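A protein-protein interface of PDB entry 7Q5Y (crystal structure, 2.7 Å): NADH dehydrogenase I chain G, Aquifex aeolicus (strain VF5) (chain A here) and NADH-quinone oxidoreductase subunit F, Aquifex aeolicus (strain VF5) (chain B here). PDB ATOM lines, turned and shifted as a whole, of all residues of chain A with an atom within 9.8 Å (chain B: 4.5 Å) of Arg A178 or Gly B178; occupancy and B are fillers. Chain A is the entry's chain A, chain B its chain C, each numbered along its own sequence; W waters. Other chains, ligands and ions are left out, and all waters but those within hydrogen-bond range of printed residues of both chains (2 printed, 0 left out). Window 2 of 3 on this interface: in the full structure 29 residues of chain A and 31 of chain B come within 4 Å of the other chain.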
ATOM      1  N   ARG A 137       2.525  -9.712  27.686  1.00  0.00           N
ATOM      2  CA  ARG A 137       3.779  -9.653  26.956  1.00  0.00           C
ATOM      3  C   ARG A 137       3.774  -8.283  26.292  1.00  0.00           C
ATOM      4  O   ARG A 137       2.712  -7.784  25.906  1.00  0.00           O
ATOM      5  CB  ARG A 137       3.945 -10.736  25.875  1.00  0.00           C
ATOM      6  CG  ARG A 137       4.297 -12.116  26.366  1.00  0.00           C
ATOM      7  CD  ARG A 137       4.610 -13.105  25.223  1.00  0.00           C
ATOM      8  NE  ARG A 137       5.921 -12.785  24.694  1.00  0.00           N
ATOM      9  CZ  ARG A 137       6.234 -12.462  23.442  1.00  0.00           C
ATOM     10  NH1 ARG A 137       5.339 -12.415  22.457  1.00  0.00           N
ATOM     11  NH2 ARG A 137       7.503 -12.193  23.180  1.00  0.00           N
ATOM     12  N   GLU A 138       4.960  -7.691  26.164  1.00  0.00           N
ATOM     13  CA  GLU A 138       5.128  -6.389  25.521  1.00  0.00           C
ATOM     14  C   GLU A 138       4.403  -6.375  24.170  1.00  0.00           C
ATOM     15  O   GLU A 138       4.404  -7.371  23.445  1.00  0.00           O
ATOM     16  CB  GLU A 138       6.637  -6.115  25.373  1.00  0.00           C
ATOM     17  CG  GLU A 138       7.039  -4.702  24.967  1.00  0.00           C
ATOM     18  CD  GLU A 138       6.624  -3.659  25.993  1.00  0.00           C
ATOM     19  OE1 GLU A 138       6.824  -3.906  27.205  1.00  0.00           O
ATOM     20  OE2 GLU A 138       6.086  -2.600  25.586  1.00  0.00           O
ATOM     21  N   HIS A 140       2.821  -3.832  20.623  1.00  0.00           N
ATOM     22  CA  HIS A 140       2.640  -2.578  19.892  1.00  0.00           C
ATOM     23  C   HIS A 140       1.575  -2.705  18.795  1.00  0.00           C
ATOM     24  O   HIS A 140       1.553  -3.671  18.022  1.00  0.00           O
ATOM     25  CB  HIS A 140       3.961  -2.101  19.303  1.00  0.00           C
ATOM     26  CG  HIS A 140       4.989  -1.801  20.347  1.00  0.00           C
ATOM     27  ND1 HIS A 140       5.877  -2.748  20.814  1.00  0.00           N
ATOM     28  CD2 HIS A 140       5.239  -0.677  21.053  1.00  0.00           C
ATOM     29  CE1 HIS A 140       6.640  -2.213  21.749  1.00  0.00           C
ATOM     30  NE2 HIS A 140       6.273  -0.957  21.911  1.00  0.00           N
ATOM     31  N   VAL A 156       6.866 -16.951  19.916  1.00  0.00           N
ATOM     32  CA  VAL A 156       7.921 -16.409  19.078  1.00  0.00           C
ATOM     33  C   VAL A 156       8.706 -17.568  18.483  1.00  0.00           C
ATOM     34  O   VAL A 156       9.519 -18.238  19.114  1.00  0.00           O
ATOM     35  CB  VAL A 156       8.788 -15.410  19.896  1.00  0.00           C
ATOM     36  CG1 VAL A 156       8.366 -15.365  21.326  1.00  0.00           C
ATOM     37  CG2 VAL A 156      10.265 -15.637  19.790  1.00  0.00           C
ATOM     38  N   TYR A 158       9.428 -16.991  14.810  1.00  0.00           N
ATOM     39  CA  TYR A 158      10.068 -16.324  13.697  1.00  0.00           C
ATOM     40  C   TYR A 158       9.631 -16.838  12.332  1.00  0.00           C
ATOM     41  O   TYR A 158      10.335 -16.632  11.348  1.00  0.00           O
ATOM     42  CB  TYR A 158      11.590 -16.402  13.857  1.00  0.00           C
ATOM     43  CG  TYR A 158      12.061 -15.902  15.222  1.00  0.00           C
ATOM     44  CD1 TYR A 158      11.979 -14.542  15.568  1.00  0.00           C
ATOM     45  CD2 TYR A 158      12.529 -16.794  16.181  1.00  0.00           C
ATOM     46  CE1 TYR A 158      12.391 -14.091  16.831  1.00  0.00           C
ATOM     47  CE2 TYR A 158      12.921 -16.362  17.440  1.00  0.00           C
ATOM     48  CZ  TYR A 158      12.873 -15.022  17.756  1.00  0.00           C
ATOM     49  OH  TYR A 158      13.295 -14.637  19.009  1.00  0.00           O
ATOM     50  N   TYR A 174       9.966  -6.724  12.030  1.00  0.00           N
ATOM     51  CA  TYR A 174      11.209  -6.784  12.784  1.00  0.00           C
ATOM     52  C   TYR A 174      10.843  -7.215  14.187  1.00  0.00           C
ATOM     53  O   TYR A 174       9.693  -7.078  14.617  1.00  0.00           O
ATOM     54  CB  TYR A 174      11.987  -5.473  12.783  1.00  0.00           C
ATOM     55  CG  TYR A 174      11.459  -4.420  13.709  1.00  0.00           C
ATOM     56  CD1 TYR A 174      11.975  -4.267  14.992  1.00  0.00           C
ATOM     57  CD2 TYR A 174      10.438  -3.561  13.294  1.00  0.00           C
ATOM     58  CE1 TYR A 174      11.482  -3.291  15.835  1.00  0.00           C
ATOM     59  CE2 TYR A 174       9.953  -2.588  14.123  1.00  0.00           C
ATOM     60  CZ  TYR A 174      10.470  -2.462  15.393  1.00  0.00           C
ATOM     61  OH  TYR A 174       9.963  -1.506  16.216  1.00  0.00           O
ATOM     62  N   VAL A 175      11.821  -7.760  14.894  1.00  0.00           N
ATOM     63  CA  VAL A 175      11.575  -8.209  16.254  1.00  0.00           C
ATOM     64  C   VAL A 175      11.927  -7.062  17.175  1.00  0.00           C
ATOM     65  O   VAL A 175      13.079  -6.614  17.193  1.00  0.00           O
ATOM     66  CB  VAL A 175      12.370  -9.470  16.599  1.00  0.00           C
ATOM     67  CG1 VAL A 175      12.184  -9.804  18.049  1.00  0.00           C
ATOM     68  CG2 VAL A 175      11.857 -10.635  15.768  1.00  0.00           C
ATOM     69  N   GLU A 176      10.926  -6.594  17.928  1.00  0.00           N
ATOM     70  CA  GLU A 176      11.060  -5.494  18.870  1.00  0.00           C
ATOM     71  C   GLU A 176      11.613  -6.139  20.121  1.00  0.00           C
ATOM     72  O   GLU A 176      11.330  -7.304  20.410  1.00  0.00           O
ATOM     73  CB  GLU A 176       9.723  -4.773  19.093  1.00  0.00           C
ATOM     74  CG  GLU A 176       9.698  -3.505  19.978  1.00  0.00           C
ATOM     75  CD  GLU A 176      10.850  -2.530  19.768  1.00  0.00           C
ATOM     76  OE1 GLU A 176      10.878  -1.805  18.732  1.00  0.00           O
ATOM     77  OE2 GLU A 176      11.754  -2.502  20.635  1.00  0.00           O
ATOM     78  N   ASP A 177      12.315  -5.334  20.898  1.00  0.00           N
ATOM     79  CA  ASP A 177      13.194  -5.660  22.001  1.00  0.00           C
ATOM     80  C   ASP A 177      13.163  -7.093  22.499  1.00  0.00           C
ATOM     81  O   ASP A 177      12.121  -7.650  22.834  1.00  0.00           O
ATOM     82  CB  ASP A 177      12.914  -4.701  23.165  1.00  0.00           C
ATOM     83  CG  ASP A 177      11.692  -5.076  23.954  1.00  0.00           C
ATOM     84  OD1 ASP A 177      10.563  -4.683  23.580  1.00  0.00           O
ATOM     85  OD2 ASP A 177      11.886  -5.780  24.960  1.00  0.00           O
ATOM     86  N   ARG A 178      14.378  -7.644  22.562  1.00  0.00           N
ATOM     87  CA  ARG A 178      14.864  -8.973  22.953  1.00  0.00           C
ATOM     88  C   ARG A 178      14.324  -9.554  24.254  1.00  0.00           C
ATOM     89  O   ARG A 178      13.663  -8.859  25.025  1.00  0.00           O
ATOM     90  CB  ARG A 178      16.402  -8.938  23.114  1.00  0.00           C
ATOM     91  CG  ARG A 178      16.877  -8.506  24.527  1.00  0.00           C
ATOM     92  CD  ARG A 178      18.372  -8.818  24.774  1.00  0.00           C
ATOM     93  NE  ARG A 178      18.901  -8.325  26.063  1.00  0.00           N
ATOM     94  CZ  ARG A 178      19.890  -7.443  26.229  1.00  0.00           C
ATOM     95  NH1 ARG A 178      20.497  -6.900  25.180  1.00  0.00           N
ATOM     96  NH2 ARG A 178      20.308  -7.126  27.458  1.00  0.00           N
ATOM     97  N   GLY A 179      14.607 -10.856  24.483  1.00  0.00           N
ATOM     98  CA  GLY A 179      14.233 -11.581  25.679  1.00  0.00           C
ATOM     99  C   GLY A 179      12.817 -12.126  25.679  1.00  0.00           C
ATOM    100  O   GLY A 179      12.191 -12.349  24.636  1.00  0.00           O
ATOM    101  N   PHE A 180      12.315 -12.362  26.893  1.00  0.00           N
ATOM    102  CA  PHE A 180      10.975 -12.909  27.025  1.00  0.00           C
ATOM    103  C   PHE A 180       9.930 -12.095  26.250  1.00  0.00           C
ATOM    104  O   PHE A 180       8.994 -12.665  25.666  1.00  0.00           O
ATOM    105  CB  PHE A 180      10.588 -12.990  28.494  1.00  0.00           C
ATOM    106  CG  PHE A 180       9.186 -13.380  28.682  1.00  0.00           C
ATOM    107  CD1 PHE A 180       8.814 -14.706  28.546  1.00  0.00           C
ATOM    108  CD2 PHE A 180       8.212 -12.415  28.924  1.00  0.00           C
ATOM    109  CE1 PHE A 180       7.495 -15.066  28.679  1.00  0.00           C
ATOM    110  CE2 PHE A 180       6.894 -12.765  29.051  1.00  0.00           C
ATOM    111  CZ  PHE A 180       6.527 -14.087  28.932  1.00  0.00           C
ATOM    112  N   HIS A 181      10.066 -10.767  26.239  1.00  0.00           N
ATOM    113  CA  HIS A 181       9.112  -9.888  25.565  1.00  0.00           C
ATOM    114  C   HIS A 181       9.393  -9.649  24.091  1.00  0.00           C
ATOM    115  O   HIS A 181       8.838  -8.696  23.538  1.00  0.00           O
ATOM    116  CB  HIS A 181       9.040  -8.534  26.272  1.00  0.00           C
ATOM    117  CG  HIS A 181       8.434  -8.622  27.632  1.00  0.00           C
ATOM    118  ND1 HIS A 181       7.075  -8.724  27.832  1.00  0.00           N
ATOM    119  CD2 HIS A 181       9.008  -8.727  28.853  1.00  0.00           C
ATOM    120  CE1 HIS A 181       6.836  -8.833  29.124  1.00  0.00           C
ATOM    121  NE2 HIS A 181       7.994  -8.851  29.765  1.00  0.00           N
ATOM    122  N   SER A 182      10.210 -10.478  23.434  1.00  0.00           N
ATOM    123  CA  SER A 182      10.425 -10.280  22.004  1.00  0.00           C
ATOM    124  C   SER A 182       9.074 -10.265  21.295  1.00  0.00           C
ATOM    125  O   SER A 182       8.341 -11.250  21.319  1.00  0.00           O
ATOM    126  CB  SER A 182      11.301 -11.390  21.433  1.00  0.00           C
ATOM    127  OG  SER A 182      12.613 -11.334  21.944  1.00  0.00           O
ATOM    128  N   ASN A 183       8.737  -9.163  20.646  1.00  0.00           N
ATOM    129  CA  ASN A 183       7.451  -9.090  19.979  1.00  0.00           C
ATOM    130  C   ASN A 183       7.601  -8.591  18.549  1.00  0.00           C
ATOM    131  O   ASN A 183       8.459  -7.767  18.256  1.00  0.00           O
ATOM    132  CB  ASN A 183       6.503  -8.174  20.769  1.00  0.00           C
ATOM    133  CG  ASN A 183       7.043  -6.771  20.922  1.00  0.00           C
ATOM    134  OD1 ASN A 183       6.802  -5.919  20.072  1.00  0.00           O
ATOM    135  ND2 ASN A 183       7.759  -6.514  22.010  1.00  0.00           N
ATOM    136  N   ILE A 184       6.749  -9.091  17.652  1.00  0.00           N
ATOM    137  CA  ILE A 184       6.815  -8.701  16.239  1.00  0.00           C
ATOM    138  C   ILE A 184       6.168  -7.329  16.019  1.00  0.00           C
ATOM    139  O   ILE A 184       5.068  -7.036  16.530  1.00  0.00           O
ATOM    140  CB  ILE A 184       6.165  -9.790  15.371  1.00  0.00           C
ATOM    141  CG1 ILE A 184       6.728 -11.173  15.756  1.00  0.00           C
ATOM    142  CG2 ILE A 184       6.295  -9.469  13.896  1.00  0.00           C
ATOM    143  CD1 ILE A 184       8.228 -11.290  15.611  1.00  0.00           C
ATOM    144  N   GLU B 137      29.607  -0.574  27.936  1.00  0.00           N
ATOM    145  CA  GLU B 137      29.775   0.091  29.223  1.00  0.00           C
ATOM    146  C   GLU B 137      31.245   0.352  29.608  1.00  0.00           C
ATOM    147  O   GLU B 137      31.514   0.733  30.756  1.00  0.00           O
ATOM    148  CB  GLU B 137      29.058  -0.716  30.304  1.00  0.00           C
ATOM    149  CG  GLU B 137      27.554  -0.832  30.064  1.00  0.00           C
ATOM    150  CD  GLU B 137      27.176  -2.005  29.152  1.00  0.00           C
ATOM    151  OE1 GLU B 137      28.062  -2.623  28.513  1.00  0.00           O
ATOM    152  OE2 GLU B 137      25.967  -2.297  29.064  1.00  0.00           O
ATOM    153  N   GLY B 176      30.189  -2.836  22.051  1.00  0.00           N
ATOM    154  CA  GLY B 176      28.921  -3.482  22.277  1.00  0.00           C
ATOM    155  C   GLY B 176      27.919  -2.406  22.649  1.00  0.00           C
ATOM    156  O   GLY B 176      28.215  -1.209  22.624  1.00  0.00           O
ATOM    157  N   ALA B 177      26.701  -2.828  22.988  1.00  0.00           N
ATOM    158  CA  ALA B 177      25.701  -1.831  23.337  1.00  0.00           C
ATOM    159  C   ALA B 177      24.780  -2.301  24.450  1.00  0.00           C
ATOM    160  O   ALA B 177      23.616  -1.883  24.520  1.00  0.00           O
ATOM    161  CB  ALA B 177      24.884  -1.434  22.108  1.00  0.00           C
ATOM    162  N   GLY B 178      25.267  -3.198  25.291  1.00  0.00           N
ATOM    163  CA  GLY B 178      24.537  -3.746  26.423  1.00  0.00           C
ATOM    164  C   GLY B 178      23.861  -5.065  26.090  1.00  0.00           C
ATOM    165  O   GLY B 178      22.693  -5.110  25.680  1.00  0.00           O
ATOM    166  N   ALA B 179      24.599  -6.143  26.269  1.00  0.00           N
ATOM    167  CA  ALA B 179      24.138  -7.502  26.042  1.00  0.00           C
ATOM    168  C   ALA B 179      25.223  -8.469  26.529  1.00  0.00           C
ATOM    169  O   ALA B 179      26.305  -8.557  25.931  1.00  0.00           O
ATOM    170  CB  ALA B 179      23.792  -7.722  24.573  1.00  0.00           C
ATOM    171  N   ARG B 196      21.649  -8.516  15.314  1.00  0.00           N
ATOM    172  CA  ARG B 196      21.290  -8.694  16.708  1.00  0.00           C
ATOM    173  C   ARG B 196      22.190  -9.792  17.263  1.00  0.00           C
ATOM    174  O   ARG B 196      22.612 -10.693  16.538  1.00  0.00           O
ATOM    175  CB  ARG B 196      19.822  -9.131  16.890  1.00  0.00           C
ATOM    176  CG  ARG B 196      18.632  -8.326  16.307  1.00  0.00           C
ATOM    177  CD  ARG B 196      17.304  -9.035  16.735  1.00  0.00           C
ATOM    178  NE  ARG B 196      16.526  -8.197  17.644  1.00  0.00           N
ATOM    179  CZ  ARG B 196      15.801  -8.636  18.668  1.00  0.00           C
ATOM    180  NH1 ARG B 196      15.747  -9.926  18.934  1.00  0.00           N
ATOM    181  NH2 ARG B 196      15.130  -7.784  19.448  1.00  0.00           N
ATOM    182  N   HIS B 344      17.338 -10.843  32.577  1.00  0.00           N
ATOM    183  CA  HIS B 344      17.697  -9.636  31.873  1.00  0.00           C
ATOM    184  C   HIS B 344      18.619  -9.872  30.694  1.00  0.00           C
ATOM    185  O   HIS B 344      18.701  -9.004  29.815  1.00  0.00           O
ATOM    186  CB  HIS B 344      18.383  -8.686  32.853  1.00  0.00           C
ATOM    187  CG  HIS B 344      18.590  -7.318  32.304  1.00  0.00           C
ATOM    188  ND1 HIS B 344      19.755  -6.940  31.679  1.00  0.00           N
ATOM    189  CD2 HIS B 344      17.765  -6.248  32.251  1.00  0.00           C
ATOM    190  CE1 HIS B 344      19.646  -5.690  31.271  1.00  0.00           C
ATOM    191  NE2 HIS B 344      18.446  -5.248  31.605  1.00  0.00           N
ATOM    192  N   GLU B 345      19.294 -11.019  30.630  1.00  0.00           N
ATOM    193  CA  GLU B 345      20.243 -11.270  29.554  1.00  0.00           C
ATOM    194  C   GLU B 345      19.833 -12.341  28.547  1.00  0.00           C
ATOM    195  O   GLU B 345      20.509 -12.473  27.524  1.00  0.00           O
ATOM    196  CB  GLU B 345      21.626 -11.626  30.145  1.00  0.00           C
ATOM    197  CG  GLU B 345      22.225 -10.494  30.993  1.00  0.00           C
ATOM    198  CD  GLU B 345      22.490  -9.192  30.235  1.00  0.00           C
ATOM    199  OE1 GLU B 345      22.526  -9.179  28.963  1.00  0.00           O
ATOM    200  OE2 GLU B 345      22.647  -8.169  30.950  1.00  0.00           O
ATOM    201  N   THR B 346      18.781 -13.117  28.794  1.00  0.00           N
ATOM    202  CA  THR B 346      18.388 -14.108  27.802  1.00  0.00           C
ATOM    203  C   THR B 346      18.055 -13.392  26.510  1.00  0.00           C
ATOM    204  O   THR B 346      17.290 -12.426  26.501  1.00  0.00           O
ATOM    205  CB  THR B 346      17.213 -14.948  28.289  1.00  0.00           C
ATOM    206  OG1 THR B 346      16.626 -15.633  27.177  1.00  0.00           O
ATOM    207  CG2 THR B 346      16.206 -14.121  29.038  1.00  0.00           C
ATOM    208  N   CYS B 347      18.649 -13.859  25.419  1.00  0.00           N
ATOM    209  CA  CYS B 347      18.468 -13.206  24.136  1.00  0.00           C
ATOM    210  C   CYS B 347      17.072 -13.412  23.550  1.00  0.00           C
ATOM    211  O   CYS B 347      16.611 -12.569  22.779  1.00  0.00           O
ATOM    212  CB  CYS B 347      19.564 -13.697  23.177  1.00  0.00           C
ATOM    213  SG  CYS B 347      19.276 -15.237  22.257  1.00  0.00           S
HETATM  214  O   HOH W   1      14.529 -12.045  20.104  1.00  0.00           O
HETATM  215  O   HOH W   2      16.711 -10.053  27.713  1.00  0.00           O
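The guanidinium group (NH2) of Arg B196 lies within hydrogen-bond range of the backbone carbonyl oxygen (O) of Val A175 (3.3 Å).
The backbone carbonyl oxygen (O) of Gly B178 is in hydrogen-bond range of the guanidinium group (NH1) of Arg A178 (2.9 Å).
The guanidinium group (NH2) of Arg A178 sits at hydrogen-bond distance from the backbone carbonyl oxygen (O) of His B344, 3.4 Å away.
The guanidinium group (NH2) of Arg A178 lies within salt-bridge range of the side-chain carboxylate (OE1) of Glu B345.
The backbone NH of Gly A179 is in hydrogen-bond range of the backbone carbonyl oxygen of Cys B347 (3.1 Å).
N of Arg A178 sits close to NH2 of Arg B196, at 3.2 Å.
The side-chain carboxylate (OE1) of Glu A176 is in hydrogen-bond range of the side-chain hydroxyl (OH) of Tyr A174.
The backbone NH (N) of Glu A176 sits at hydrogen-bond distance from the backbone carbonyl oxygen (O) of Asn A183 (2.8 Å).
O of Asp A177 lies close to N of Ser A182 (3.5 Å).
The backbone carbonyl oxygen (O) of Gly A179 is in hydrogen-bond range of the side-chain hydroxyl (OG) of Ser A182, 2.9 Å away.
A ring nitrogen (ND1) of His B344 sits at hydrogen-bond distance from the side-chain carboxylate (OE2) of Glu B345.
Among the printed residues, pairs that only touch across the chains: Glu A176 with Arg B196, Asp A177 with Arg B196, Arg A178 with Ala B179, Arg A178 with Cys B347 and Gly A179 with Thr B346.
Of the printed residues of chain B, Glu A176 touches Arg B196 (3.9 Å).
Of the printed residues of chain B, Arg A178 touches Gly B178, Ala B179, Arg B196, His B344, Glu B345 and Cys B347.
Of the printed residues of chain B, Gly A179 touches Thr B346 (3.3 Å) and Cys B347 (3.1 Å).
Of chain A, only Arg A178 comes within 4 Å of Gly B178.
Of the printed residues of chain A, Cys B347 touches Arg A178 and Gly A179.
The nearest residue of chain B that does not touch Arg A178 is Thr B346 (4.1 Å).
Printed residues of chain A that touch a printed residue of chain B: Val A175, Glu A176, Asp A177, Arg A178 and Gly A179.
Along chain A the printed residues that touch a printed residue of chain B span positions 175 to 179.
Hydrophobic or aromatic side chains of chain B within 4 Å of the printed part of chain A: Ala B179.
Water W1 lies within hydrogen-bond range of the guanidinium group (NH1) of Arg B196 (2.7 Å), the side-chain hydroxyl (OG) of Ser A182 (2.7 Å), the side-chain hydroxyl (OH) of Tyr A158 (3.1 Å) and the backbone carbonyl oxygen (O) of Cys B347 (3.4 Å).
Water W2 lies within hydrogen-bond range of the backbone carbonyl oxygen of Thr B346 (2.7 Å), the backbone carbonyl oxygen of His B344 (3.1 Å) and the guanidinium group of Arg A178 (3.2 Å).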
